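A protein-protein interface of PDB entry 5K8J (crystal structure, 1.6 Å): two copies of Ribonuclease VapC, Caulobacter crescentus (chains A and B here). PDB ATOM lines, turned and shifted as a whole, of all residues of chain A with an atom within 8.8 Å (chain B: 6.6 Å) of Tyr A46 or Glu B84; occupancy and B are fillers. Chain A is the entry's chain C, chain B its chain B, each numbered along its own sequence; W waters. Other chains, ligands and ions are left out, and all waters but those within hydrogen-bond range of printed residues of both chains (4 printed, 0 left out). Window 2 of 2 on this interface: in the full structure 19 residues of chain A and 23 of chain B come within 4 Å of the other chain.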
ATOM      1  N   ARG A  14       7.027 -12.021  29.861  1.00  0.00           N
ATOM      2  CA  ARG A  14       6.279 -12.690  28.809  1.00  0.00           C
ATOM      3  C   ARG A  14       5.611 -11.691  27.883  1.00  0.00           C
ATOM      4  O   ARG A  14       5.601 -11.860  26.657  1.00  0.00           O
ATOM      5  CB  ARG A  14       5.210 -13.571  29.430  1.00  0.00           C
ATOM      6  CG  ARG A  14       4.680 -14.684  28.493  1.00  0.00           C
ATOM      7  CD  ARG A  14       3.469 -14.225  27.756  1.00  0.00           C
ATOM      8  NE  ARG A  14       2.524 -13.658  28.707  1.00  0.00           N
ATOM      9  CZ  ARG A  14       1.704 -14.361  29.449  1.00  0.00           C
ATOM     10  NH1 ARG A  14       1.664 -15.689  29.329  1.00  0.00           N
ATOM     11  NH2 ARG A  14       0.899 -13.737  30.281  1.00  0.00           N
ATOM     12  N   ARG A  38       5.212 -21.227  36.495  1.00  0.00           N
ATOM     13  CA  ARG A  38       4.797 -21.900  35.278  1.00  0.00           C
ATOM     14  C   ARG A  38       3.334 -22.323  35.372  1.00  0.00           C
ATOM     15  O   ARG A  38       2.566 -22.105  34.447  1.00  0.00           O
ATOM     16  CB  ARG A  38       5.674 -23.116  34.962  1.00  0.00           C
ATOM     17  CG  ARG A  38       5.151 -23.875  33.751  1.00  0.00           C
ATOM     18  CD  ARG A  38       5.998 -25.043  33.292  1.00  0.00           C
ATOM     19  NE  ARG A  38       5.210 -25.683  32.267  1.00  0.00           N
ATOM     20  CZ  ARG A  38       5.351 -26.923  31.813  1.00  0.00           C
ATOM     21  NH1 ARG A  38       6.322 -27.700  32.237  1.00  0.00           N
ATOM     22  NH2 ARG A  38       4.486 -27.375  30.929  1.00  0.00           N
ATOM     23  N   VAL A  39       2.952 -22.969  36.484  1.00  0.00           N
ATOM     24  CA  VAL A  39       1.554 -23.380  36.684  1.00  0.00           C
ATOM     25  C   VAL A  39       0.601 -22.193  36.539  1.00  0.00           C
ATOM     26  O   VAL A  39      -0.417 -22.277  35.828  1.00  0.00           O
ATOM     27  CB  VAL A  39       1.383 -24.090  38.041  1.00  0.00           C
ATOM     28  CG1 VAL A  39      -0.134 -24.276  38.377  1.00  0.00           C
ATOM     29  CG2 VAL A  39       2.073 -25.432  37.997  1.00  0.00           C
ATOM     30  N   GLU A  40       0.921 -21.071  37.184  1.00  0.00           N
ATOM     31  CA  GLU A  40       0.075 -19.884  37.077  1.00  0.00           C
ATOM     32  C   GLU A  40      -0.059 -19.440  35.631  1.00  0.00           C
ATOM     33  O   GLU A  40      -1.161 -19.130  35.164  1.00  0.00           O
ATOM     34  CB  GLU A  40       0.646 -18.765  37.943  1.00  0.00           C
ATOM     35  CG  GLU A  40       0.661 -19.078  39.421  1.00  0.00           C
ATOM     36  CD  GLU A  40       0.998 -17.885  40.253  1.00  0.00           C
ATOM     37  OE1 GLU A  40       2.138 -17.816  40.731  1.00  0.00           O
ATOM     38  OE2 GLU A  40       0.130 -16.980  40.409  1.00  0.00           O
ATOM     39  N   LEU A  41       1.066 -19.376  34.908  1.00  0.00           N
ATOM     40  CA  LEU A  41       1.042 -18.901  33.533  1.00  0.00           C
ATOM     41  C   LEU A  41       0.314 -19.871  32.610  1.00  0.00           C
ATOM     42  O   LEU A  41      -0.353 -19.452  31.655  1.00  0.00           O
ATOM     43  CB  LEU A  41       2.473 -18.644  33.074  1.00  0.00           C
ATOM     44  CG  LEU A  41       3.236 -17.515  33.780  1.00  0.00           C
ATOM     45  CD1 LEU A  41       4.737 -17.791  33.811  1.00  0.00           C
ATOM     46  CD2 LEU A  41       3.019 -16.249  33.054  1.00  0.00           C
ATOM     47  N   GLU A  42       0.464 -21.175  32.840  1.00  0.00           N
ATOM     48  CA  GLU A  42      -0.254 -22.137  32.009  1.00  0.00           C
ATOM     49  C   GLU A  42      -1.758 -21.933  32.133  1.00  0.00           C
ATOM     50  O   GLU A  42      -2.486 -21.964  31.128  1.00  0.00           O
ATOM     51  CB  GLU A  42       0.119 -23.584  32.393  1.00  0.00           C
ATOM     52  CG  GLU A  42       1.597 -24.007  32.227  1.00  0.00           C
ATOM     53  CD  GLU A  42       1.957 -24.337  30.812  1.00  0.00           C
ATOM     54  OE1 GLU A  42       1.088 -24.164  29.930  1.00  0.00           O
ATOM     55  OE2 GLU A  42       3.109 -24.796  30.572  1.00  0.00           O
ATOM     56  N   GLY A  43      -2.239 -21.718  33.358  1.00  0.00           N
ATOM     57  CA  GLY A  43      -3.657 -21.435  33.542  1.00  0.00           C
ATOM     58  C   GLY A  43      -4.056 -20.116  32.902  1.00  0.00           C
ATOM     59  O   GLY A  43      -5.110 -20.011  32.269  1.00  0.00           O
ATOM     60  N   GLY A  44      -3.174 -19.120  32.993  1.00  0.00           N
ATOM     61  CA  GLY A  44      -3.473 -17.807  32.462  1.00  0.00           C
ATOM     62  C   GLY A  44      -3.694 -17.816  30.970  1.00  0.00           C
ATOM     63  O   GLY A  44      -4.393 -16.955  30.434  1.00  0.00           O
ATOM     64  N   VAL A  45      -3.121 -18.791  30.270  1.00  0.00           N
ATOM     65  CA  VAL A  45      -3.382 -18.881  28.839  1.00  0.00           C
ATOM     66  C   VAL A  45      -4.879 -18.926  28.576  1.00  0.00           C
ATOM     67  O   VAL A  45      -5.386 -18.286  27.648  1.00  0.00           O
ATOM     68  CB  VAL A  45      -2.686 -20.111  28.224  1.00  0.00           C
ATOM     69  CG1 VAL A  45      -3.175 -20.332  26.773  1.00  0.00           C
ATOM     70  CG2 VAL A  45      -1.176 -19.939  28.286  1.00  0.00           C
ATOM     71  N   TYR A  46      -5.613 -19.666  29.412  1.00  0.00           N
ATOM     72  CA  TYR A  46      -7.035 -19.907  29.219  1.00  0.00           C
ATOM     73  C   TYR A  46      -7.920 -19.003  30.084  1.00  0.00           C
ATOM     74  O   TYR A  46      -9.143 -19.208  30.138  1.00  0.00           O
ATOM     75  CB  TYR A  46      -7.319 -21.397  29.468  1.00  0.00           C
ATOM     76  CG  TYR A  46      -6.563 -22.208  28.438  1.00  0.00           C
ATOM     77  CD1 TYR A  46      -7.017 -22.282  27.137  1.00  0.00           C
ATOM     78  CD2 TYR A  46      -5.353 -22.813  28.739  1.00  0.00           C
ATOM     79  CE1 TYR A  46      -6.307 -22.957  26.171  1.00  0.00           C
ATOM     80  CE2 TYR A  46      -4.639 -23.496  27.775  1.00  0.00           C
ATOM     81  CZ  TYR A  46      -5.129 -23.558  26.490  1.00  0.00           C
ATOM     82  OH  TYR A  46      -4.425 -24.203  25.510  1.00  0.00           O
ATOM     83  N   ARG A  47      -7.340 -17.971  30.697  1.00  0.00           N
ATOM     84  CA  ARG A  47      -8.098 -17.080  31.576  1.00  0.00           C
ATOM     85  C   ARG A  47      -9.137 -16.288  30.795  1.00  0.00           C
ATOM     86  O   ARG A  47     -10.243 -16.039  31.291  1.00  0.00           O
ATOM     87  CB  ARG A  47      -7.142 -16.143  32.310  1.00  0.00           C
ATOM     88  CG  ARG A  47      -7.788 -15.318  33.397  1.00  0.00           C
ATOM     89  CD  ARG A  47      -6.747 -14.475  34.134  1.00  0.00           C
ATOM     90  NE  ARG A  47      -6.319 -13.334  33.326  1.00  0.00           N
ATOM     91  CZ  ARG A  47      -6.949 -12.160  33.274  1.00  0.00           C
ATOM     92  NH1 ARG A  47      -8.048 -11.946  33.992  1.00  0.00           N
ATOM     93  NH2 ARG A  47      -6.478 -11.190  32.499  1.00  0.00           N
ATOM     94  N   GLU A  48      -8.807 -15.890  29.574  1.00  0.00           N
ATOM     95  CA  GLU A  48      -9.764 -15.264  28.674  1.00  0.00           C
ATOM     96  C   GLU A  48      -9.423 -15.714  27.271  1.00  0.00           C
ATOM     97  O   GLU A  48      -8.314 -16.174  27.009  1.00  0.00           O
ATOM     98  CB  GLU A  48      -9.743 -13.730  28.758  1.00  0.00           C
ATOM     99  CG  GLU A  48      -8.352 -13.130  28.894  1.00  0.00           C
ATOM    100  CD  GLU A  48      -8.359 -11.617  28.820  1.00  0.00           C
ATOM    101  OE1 GLU A  48      -7.283 -11.024  28.595  1.00  0.00           O
ATOM    102  OE2 GLU A  48      -9.443 -11.018  28.981  1.00  0.00           O
ATOM    103  N   ALA A  49     -10.388 -15.586  26.362  1.00  0.00           N
ATOM    104  CA  ALA A  49     -10.125 -15.954  24.976  1.00  0.00           C
ATOM    105  C   ALA A  49      -9.253 -14.917  24.283  1.00  0.00           C
ATOM    106  O   ALA A  49      -8.418 -15.278  23.439  1.00  0.00           O
ATOM    107  CB  ALA A  49     -11.443 -16.138  24.216  1.00  0.00           C
ATOM    108  N   ALA A  50      -9.407 -13.644  24.659  1.00  0.00           N
ATOM    109  CA  ALA A  50      -8.682 -12.558  24.007  1.00  0.00           C
ATOM    110  C   ALA A  50      -7.175 -12.723  24.187  1.00  0.00           C
ATOM    111  O   ALA A  50      -6.668 -12.719  25.314  1.00  0.00           O
ATOM    112  CB  ALA A  50      -9.138 -11.214  24.572  1.00  0.00           C
ATOM    113  N   GLN A  51      -6.473 -12.882  23.065  1.00  0.00           N
ATOM    114  CA  GLN A  51      -5.015 -12.927  23.005  1.00  0.00           C
ATOM    115  C   GLN A  51      -4.436 -14.133  23.730  1.00  0.00           C
ATOM    116  O   GLN A  51      -3.259 -14.135  24.104  1.00  0.00           O
ATOM    117  CB  GLN A  51      -4.420 -11.624  23.540  1.00  0.00           C
ATOM    118  CG  GLN A  51      -5.047 -10.398  22.852  1.00  0.00           C
ATOM    119  CD  GLN A  51      -4.090  -9.237  22.697  1.00  0.00           C
ATOM    120  OE1 GLN A  51      -3.693  -8.606  23.679  1.00  0.00           O
ATOM    121  NE2 GLN A  51      -3.718  -8.942  21.455  1.00  0.00           N
ATOM    122  N   ALA A  52      -5.244 -15.180  23.893  1.00  0.00           N
ATOM    123  CA  ALA A  52      -4.746 -16.421  24.470  1.00  0.00           C
ATOM    124  C   ALA A  52      -3.610 -17.009  23.631  1.00  0.00           C
ATOM    125  O   ALA A  52      -2.648 -17.562  24.178  1.00  0.00           O
ATOM    126  CB  ALA A  52      -5.904 -17.415  24.599  1.00  0.00           C
ATOM    127  N   GLY A  53      -3.698 -16.890  22.302  1.00  0.00           N
ATOM    128  CA  GLY A  53      -2.628 -17.395  21.453  1.00  0.00           C
ATOM    129  C   GLY A  53      -1.288 -16.732  21.714  1.00  0.00           C
ATOM    130  O   GLY A  53      -0.242 -17.389  21.693  1.00  0.00           O
ATOM    131  N   ARG A  55      -0.447 -15.218  24.589  1.00  0.00           N
ATOM    132  CA  ARG A  55       0.000 -15.651  25.898  1.00  0.00           C
ATOM    133  C   ARG A  55       0.653 -17.027  25.802  1.00  0.00           C
ATOM    134  O   ARG A  55       1.678 -17.282  26.447  1.00  0.00           O
ATOM    135  CB  ARG A  55      -1.184 -15.649  26.880  1.00  0.00           C
ATOM    136  CG  ARG A  55      -1.601 -14.240  27.334  1.00  0.00           C
ATOM    137  CD  ARG A  55      -2.445 -14.274  28.643  1.00  0.00           C
ATOM    138  NE  ARG A  55      -3.703 -14.990  28.426  1.00  0.00           N
ATOM    139  CZ  ARG A  55      -4.733 -14.506  27.743  1.00  0.00           C
ATOM    140  NH1 ARG A  55      -4.677 -13.295  27.190  1.00  0.00           N
ATOM    141  NH2 ARG A  55      -5.821 -15.246  27.589  1.00  0.00           N
ATOM    142  N   ARG A  56       0.096 -17.908  24.956  1.00  0.00           N
ATOM    143  CA  ARG A  56       0.600 -19.277  24.840  1.00  0.00           C
ATOM    144  C   ARG A  56       1.956 -19.322  24.146  1.00  0.00           C
ATOM    145  O   ARG A  56       2.898 -19.941  24.651  1.00  0.00           O
ATOM    146  CB  ARG A  56      -0.392 -20.143  24.080  1.00  0.00           C
ATOM    147  CG  ARG A  56       0.155 -21.572  23.847  1.00  0.00           C
ATOM    148  CD  ARG A  56      -0.739 -22.450  23.050  1.00  0.00           C
ATOM    149  NE  ARG A  56      -2.131 -22.446  23.497  1.00  0.00           N
ATOM    150  CZ  ARG A  56      -3.116 -21.756  22.920  1.00  0.00           C
ATOM    151  NH1 ARG A  56      -2.882 -20.985  21.864  1.00  0.00           N
ATOM    152  NH2 ARG A  56      -4.344 -21.838  23.411  1.00  0.00           N
ATOM    153  N   LEU A  59       4.673 -17.557  26.258  1.00  0.00           N
ATOM    154  CA  LEU A  59       4.985 -18.388  27.411  1.00  0.00           C
ATOM    155  C   LEU A  59       5.898 -19.527  27.008  1.00  0.00           C
ATOM    156  O   LEU A  59       6.900 -19.807  27.681  1.00  0.00           O
ATOM    157  CB  LEU A  59       3.700 -18.959  28.030  1.00  0.00           C
ATOM    158  CG  LEU A  59       3.951 -19.968  29.157  1.00  0.00           C
ATOM    159  CD1 LEU A  59       4.704 -19.315  30.301  1.00  0.00           C
ATOM    160  CD2 LEU A  59       2.629 -20.550  29.664  1.00  0.00           C
ATOM    161  N   ASP A  60       5.561 -20.218  25.923  1.00  0.00           N
ATOM    162  CA  ASP A  60       6.311 -21.419  25.610  1.00  0.00           C
ATOM    163  C   ASP A  60       7.764 -21.107  25.250  1.00  0.00           C
ATOM    164  O   ASP A  60       8.661 -21.877  25.605  1.00  0.00           O
ATOM    165  CB  ASP A  60       5.587 -22.175  24.492  1.00  0.00           C
ATOM    166  CG  ASP A  60       4.281 -22.820  24.985  1.00  0.00           C
ATOM    167  OD1 ASP A  60       4.073 -22.917  26.236  1.00  0.00           O
ATOM    168  OD2 ASP A  60       3.458 -23.220  24.126  1.00  0.00           O
ATOM    169  N   TYR B  79      -0.685 -30.565  34.135  1.00  0.00           N
ATOM    170  CA  TYR B  79      -1.514 -29.421  34.472  1.00  0.00           C
ATOM    171  C   TYR B  79      -1.908 -28.663  33.219  1.00  0.00           C
ATOM    172  O   TYR B  79      -3.061 -28.267  33.065  1.00  0.00           O
ATOM    173  CB  TYR B  79      -0.794 -28.490  35.473  1.00  0.00           C
ATOM    174  CG  TYR B  79      -1.630 -27.311  35.898  1.00  0.00           C
ATOM    175  CD1 TYR B  79      -2.451 -27.384  37.025  1.00  0.00           C
ATOM    176  CD2 TYR B  79      -1.643 -26.130  35.157  1.00  0.00           C
ATOM    177  CE1 TYR B  79      -3.258 -26.332  37.393  1.00  0.00           C
ATOM    178  CE2 TYR B  79      -2.452 -25.066  35.531  1.00  0.00           C
ATOM    179  CZ  TYR B  79      -3.257 -25.181  36.659  1.00  0.00           C
ATOM    180  OH  TYR B  79      -4.086 -24.167  37.061  1.00  0.00           O
ATOM    181  N   ARG B  80      -0.965 -28.468  32.300  1.00  0.00           N
ATOM    182  CA  ARG B  80      -1.299 -27.796  31.047  1.00  0.00           C
ATOM    183  C   ARG B  80      -2.385 -28.550  30.311  1.00  0.00           C
ATOM    184  O   ARG B  80      -3.344 -27.949  29.822  1.00  0.00           O
ATOM    185  CB  ARG B  80      -0.042 -27.641  30.192  1.00  0.00           C
ATOM    186  CG  ARG B  80      -0.299 -27.125  28.763  1.00  0.00           C
ATOM    187  CD  ARG B  80       1.025 -27.051  27.946  1.00  0.00           C
ATOM    188  NE  ARG B  80       1.549 -28.392  27.704  1.00  0.00           N
ATOM    189  CZ  ARG B  80       2.824 -28.689  27.467  1.00  0.00           C
ATOM    190  NH1 ARG B  80       3.754 -27.738  27.451  1.00  0.00           N
ATOM    191  NH2 ARG B  80       3.165 -29.956  27.255  1.00  0.00           N
ATOM    192  N   ARG B  81      -2.260 -29.878  30.209  1.00  0.00           N
ATOM    193  CA  ARG B  81      -3.313 -30.636  29.533  1.00  0.00           C
ATOM    194  C   ARG B  81      -4.653 -30.504  30.247  1.00  0.00           C
ATOM    195  O   ARG B  81      -5.707 -30.482  29.605  1.00  0.00           O
ATOM    196  CB  ARG B  81      -2.898 -32.100  29.406  1.00  0.00           C
ATOM    197  CG  ARG B  81      -1.783 -32.282  28.349  1.00  0.00           C
ATOM    198  CD  ARG B  81      -1.566 -33.747  27.978  1.00  0.00           C
ATOM    199  NE  ARG B  81      -0.877 -34.439  29.057  1.00  0.00           N
ATOM    200  CZ  ARG B  81       0.446 -34.481  29.172  1.00  0.00           C
ATOM    201  NH1 ARG B  81       1.225 -33.880  28.276  1.00  0.00           N
ATOM    202  NH2 ARG B  81       1.000 -35.106  30.193  1.00  0.00           N
ATOM    203  N   ILE B  82      -4.648 -30.450  31.580  1.00  0.00           N
ATOM    204  CA  ILE B  82      -5.902 -30.277  32.312  1.00  0.00           C
ATOM    205  C   ILE B  82      -6.582 -28.966  31.936  1.00  0.00           C
ATOM    206  O   ILE B  82      -7.769 -28.941  31.622  1.00  0.00           O
ATOM    207  CB  ILE B  82      -5.666 -30.339  33.830  1.00  0.00           C
ATOM    208  CG1 ILE B  82      -5.235 -31.736  34.259  1.00  0.00           C
ATOM    209  CG2 ILE B  82      -6.920 -29.946  34.545  1.00  0.00           C
ATOM    210  CD1 ILE B  82      -4.836 -31.869  35.771  1.00  0.00           C
ATOM    211  N   VAL B  83      -5.853 -27.843  31.989  1.00  0.00           N
ATOM    212  CA  VAL B  83      -6.508 -26.577  31.680  1.00  0.00           C
ATOM    213  C   VAL B  83      -6.840 -26.469  30.191  1.00  0.00           C
ATOM    214  O   VAL B  83      -7.817 -25.808  29.822  1.00  0.00           O
ATOM    215  CB  VAL B  83      -5.679 -25.369  32.175  1.00  0.00           C
ATOM    216  CG1 VAL B  83      -5.616 -25.340  33.718  1.00  0.00           C
ATOM    217  CG2 VAL B  83      -4.257 -25.341  31.572  1.00  0.00           C
ATOM    218  N   GLU B  84      -6.074 -27.139  29.311  1.00  0.00           N
ATOM    219  CA  GLU B  84      -6.422 -27.136  27.888  1.00  0.00           C
ATOM    220  C   GLU B  84      -7.801 -27.716  27.658  1.00  0.00           C
ATOM    221  O   GLU B  84      -8.523 -27.316  26.723  1.00  0.00           O
ATOM    222  CB  GLU B  84      -5.407 -27.953  27.073  1.00  0.00           C
ATOM    223  CG  GLU B  84      -4.122 -27.245  26.770  1.00  0.00           C
ATOM    224  CD  GLU B  84      -3.132 -28.127  26.010  1.00  0.00           C
ATOM    225  OE1 GLU B  84      -3.421 -29.339  25.732  1.00  0.00           O
ATOM    226  OE2 GLU B  84      -2.076 -27.591  25.642  1.00  0.00           O
ATOM    227  N   SER B  85      -8.162 -28.699  28.465  1.00  0.00           N
ATOM    228  CA  SER B  85      -9.444 -29.368  28.354  1.00  0.00           C
ATOM    229  C   SER B  85     -10.538 -28.692  29.179  1.00  0.00           C
ATOM    230  O   SER B  85     -11.636 -28.422  28.679  1.00  0.00           O
ATOM    231  CB  SER B  85      -9.303 -30.814  28.821  1.00  0.00           C
ATOM    232  OG  SER B  85     -10.504 -31.500  28.527  1.00  0.00           O
ATOM    233  N   ALA B  86     -10.258 -28.429  30.434  1.00  0.00           N
ATOM    234  CA  ALA B  86     -11.294 -28.003  31.359  1.00  0.00           C
ATOM    235  C   ALA B  86     -11.433 -26.491  31.453  1.00  0.00           C
ATOM    236  O   ALA B  86     -12.408 -26.008  32.057  1.00  0.00           O
ATOM    237  CB  ALA B  86     -10.972 -28.557  32.749  1.00  0.00           C
ATOM    238  N   GLY B  87     -10.464 -25.745  30.935  1.00  0.00           N
ATOM    239  CA  GLY B  87     -10.428 -24.316  31.110  1.00  0.00           C
ATOM    240  C   GLY B  87      -9.756 -23.959  32.414  1.00  0.00           C
ATOM    241  O   GLY B  87      -9.333 -24.809  33.192  1.00  0.00           O
ATOM    242  N   TYR B  88      -9.664 -22.662  32.658  1.00  0.00           N
ATOM    243  CA  TYR B  88      -8.967 -22.155  33.824  1.00  0.00           C
ATOM    244  C   TYR B  88      -9.904 -22.015  35.017  1.00  0.00           C
ATOM    245  O   TYR B  88     -11.023 -21.505  34.897  1.00  0.00           O
ATOM    246  CB  TYR B  88      -8.367 -20.794  33.516  1.00  0.00           C
ATOM    247  CG  TYR B  88      -7.696 -20.148  34.695  1.00  0.00           C
ATOM    248  CD1 TYR B  88      -6.632 -20.776  35.373  1.00  0.00           C
ATOM    249  CD2 TYR B  88      -8.124 -18.913  35.148  1.00  0.00           C
ATOM    250  CE1 TYR B  88      -6.020 -20.175  36.453  1.00  0.00           C
ATOM    251  CE2 TYR B  88      -7.505 -18.299  36.241  1.00  0.00           C
ATOM    252  CZ  TYR B  88      -6.454 -18.926  36.870  1.00  0.00           C
ATOM    253  OH  TYR B  88      -5.848 -18.316  37.942  1.00  0.00           O
HETATM  254  O   HOH W   1      -3.022 -17.608  36.500  1.00  0.00           O
HETATM  255  O   HOH W   2       4.138 -25.130  28.173  1.00  0.00           O
HETATM  256  O   HOH W   3     -11.010 -21.040  30.650  1.00  0.00           O
HETATM  257  O   HOH W   4      -2.972 -21.857  36.886  1.00  0.00           O
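NE of Arg A38 lies within salt-bridge range of OE2 of Glu A42. The side-chain hydroxyl of Tyr A46 lies within hydrogen-bond range of the guanidinium group of Arg A56, at 3.2 Å.
NH2 of Arg A38 touches NH1 of Arg B80, 3.6 Å away. Val A39 touches Tyr B79 (O to CE2, 3.5 Å). Glu A42 touches Arg B80. Val B83 touches Glu A42. CE2 of Tyr B79 touches N of Gly A43 (3.997 Å). Tyr B88 touches Gly A43. Tyr A46 touches Val B83. Tyr A46 touches Glu B84. CB of Tyr B88 touches O of Tyr A46, at 3.8 Å.
Tyr A46 touches just these residues of chain B: Val B83 (3.95 Å), Glu B84 (3.3 Å) and Tyr B88 (3.8 Å). Printed residues of chain A within 4 Å of Glu B84: Tyr A46. No residue of chain A comes within 4 Å of Ser B85. Printed residues of chain B within 4 Å of Arg A38: Arg B80. Of the printed residues of chain B, Gly A43 touches Tyr B79 and Tyr B88. Printed residues of chain A within 4 Å of Tyr B79: Val A39 (3.5 Å) and Gly A43 (3.997 Å). Arg B81 touches none of the printed residues of chain A. Arg A56 touches none of the printed residues of chain B. The nearest residue of chain A that does not touch Glu B84 is Arg A56 (5.6 Å).
Of the 21 printed residues of chain A, 5 touch a printed residue of chain B. Hydrophobic or aromatic side chains of chain A that line the printed part of chain B: Val A39 and Tyr A46. Of the 10 printed residues of chain B, 5 touch a printed residue of chain A. Hydrophobic or aromatic side chains of chain B that line the printed part of chain A: Tyr B79, Val B83 and Tyr B88.
No position is printed for both chains. Of the 9 pairs that touch across the chains among the printed residues, none has its exchanged pair printed and touching as well.
Water W4 bridges the side-chain hydroxyl of Tyr B79 (2.6 Å) and the backbone carbonyl oxygen of Val A39 (2.8 Å). Water W2 lies within hydrogen-bond range of OE2 of Glu A42 (2.6 Å), NH1 of Arg B80 (2.7 Å) and OD1 of Asp A60 (2.9 Å). Water W3 lies within hydrogen-bond range of the backbone carbonyl oxygen (O) of Tyr A46 (2.7 Å) and the backbone NH (N) of Tyr B88 (2.9 Å). Water W1 lies within hydrogen-bond range of O of Glu A40 (2.8 Å) and OH of Tyr B88 (3.3 Å).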
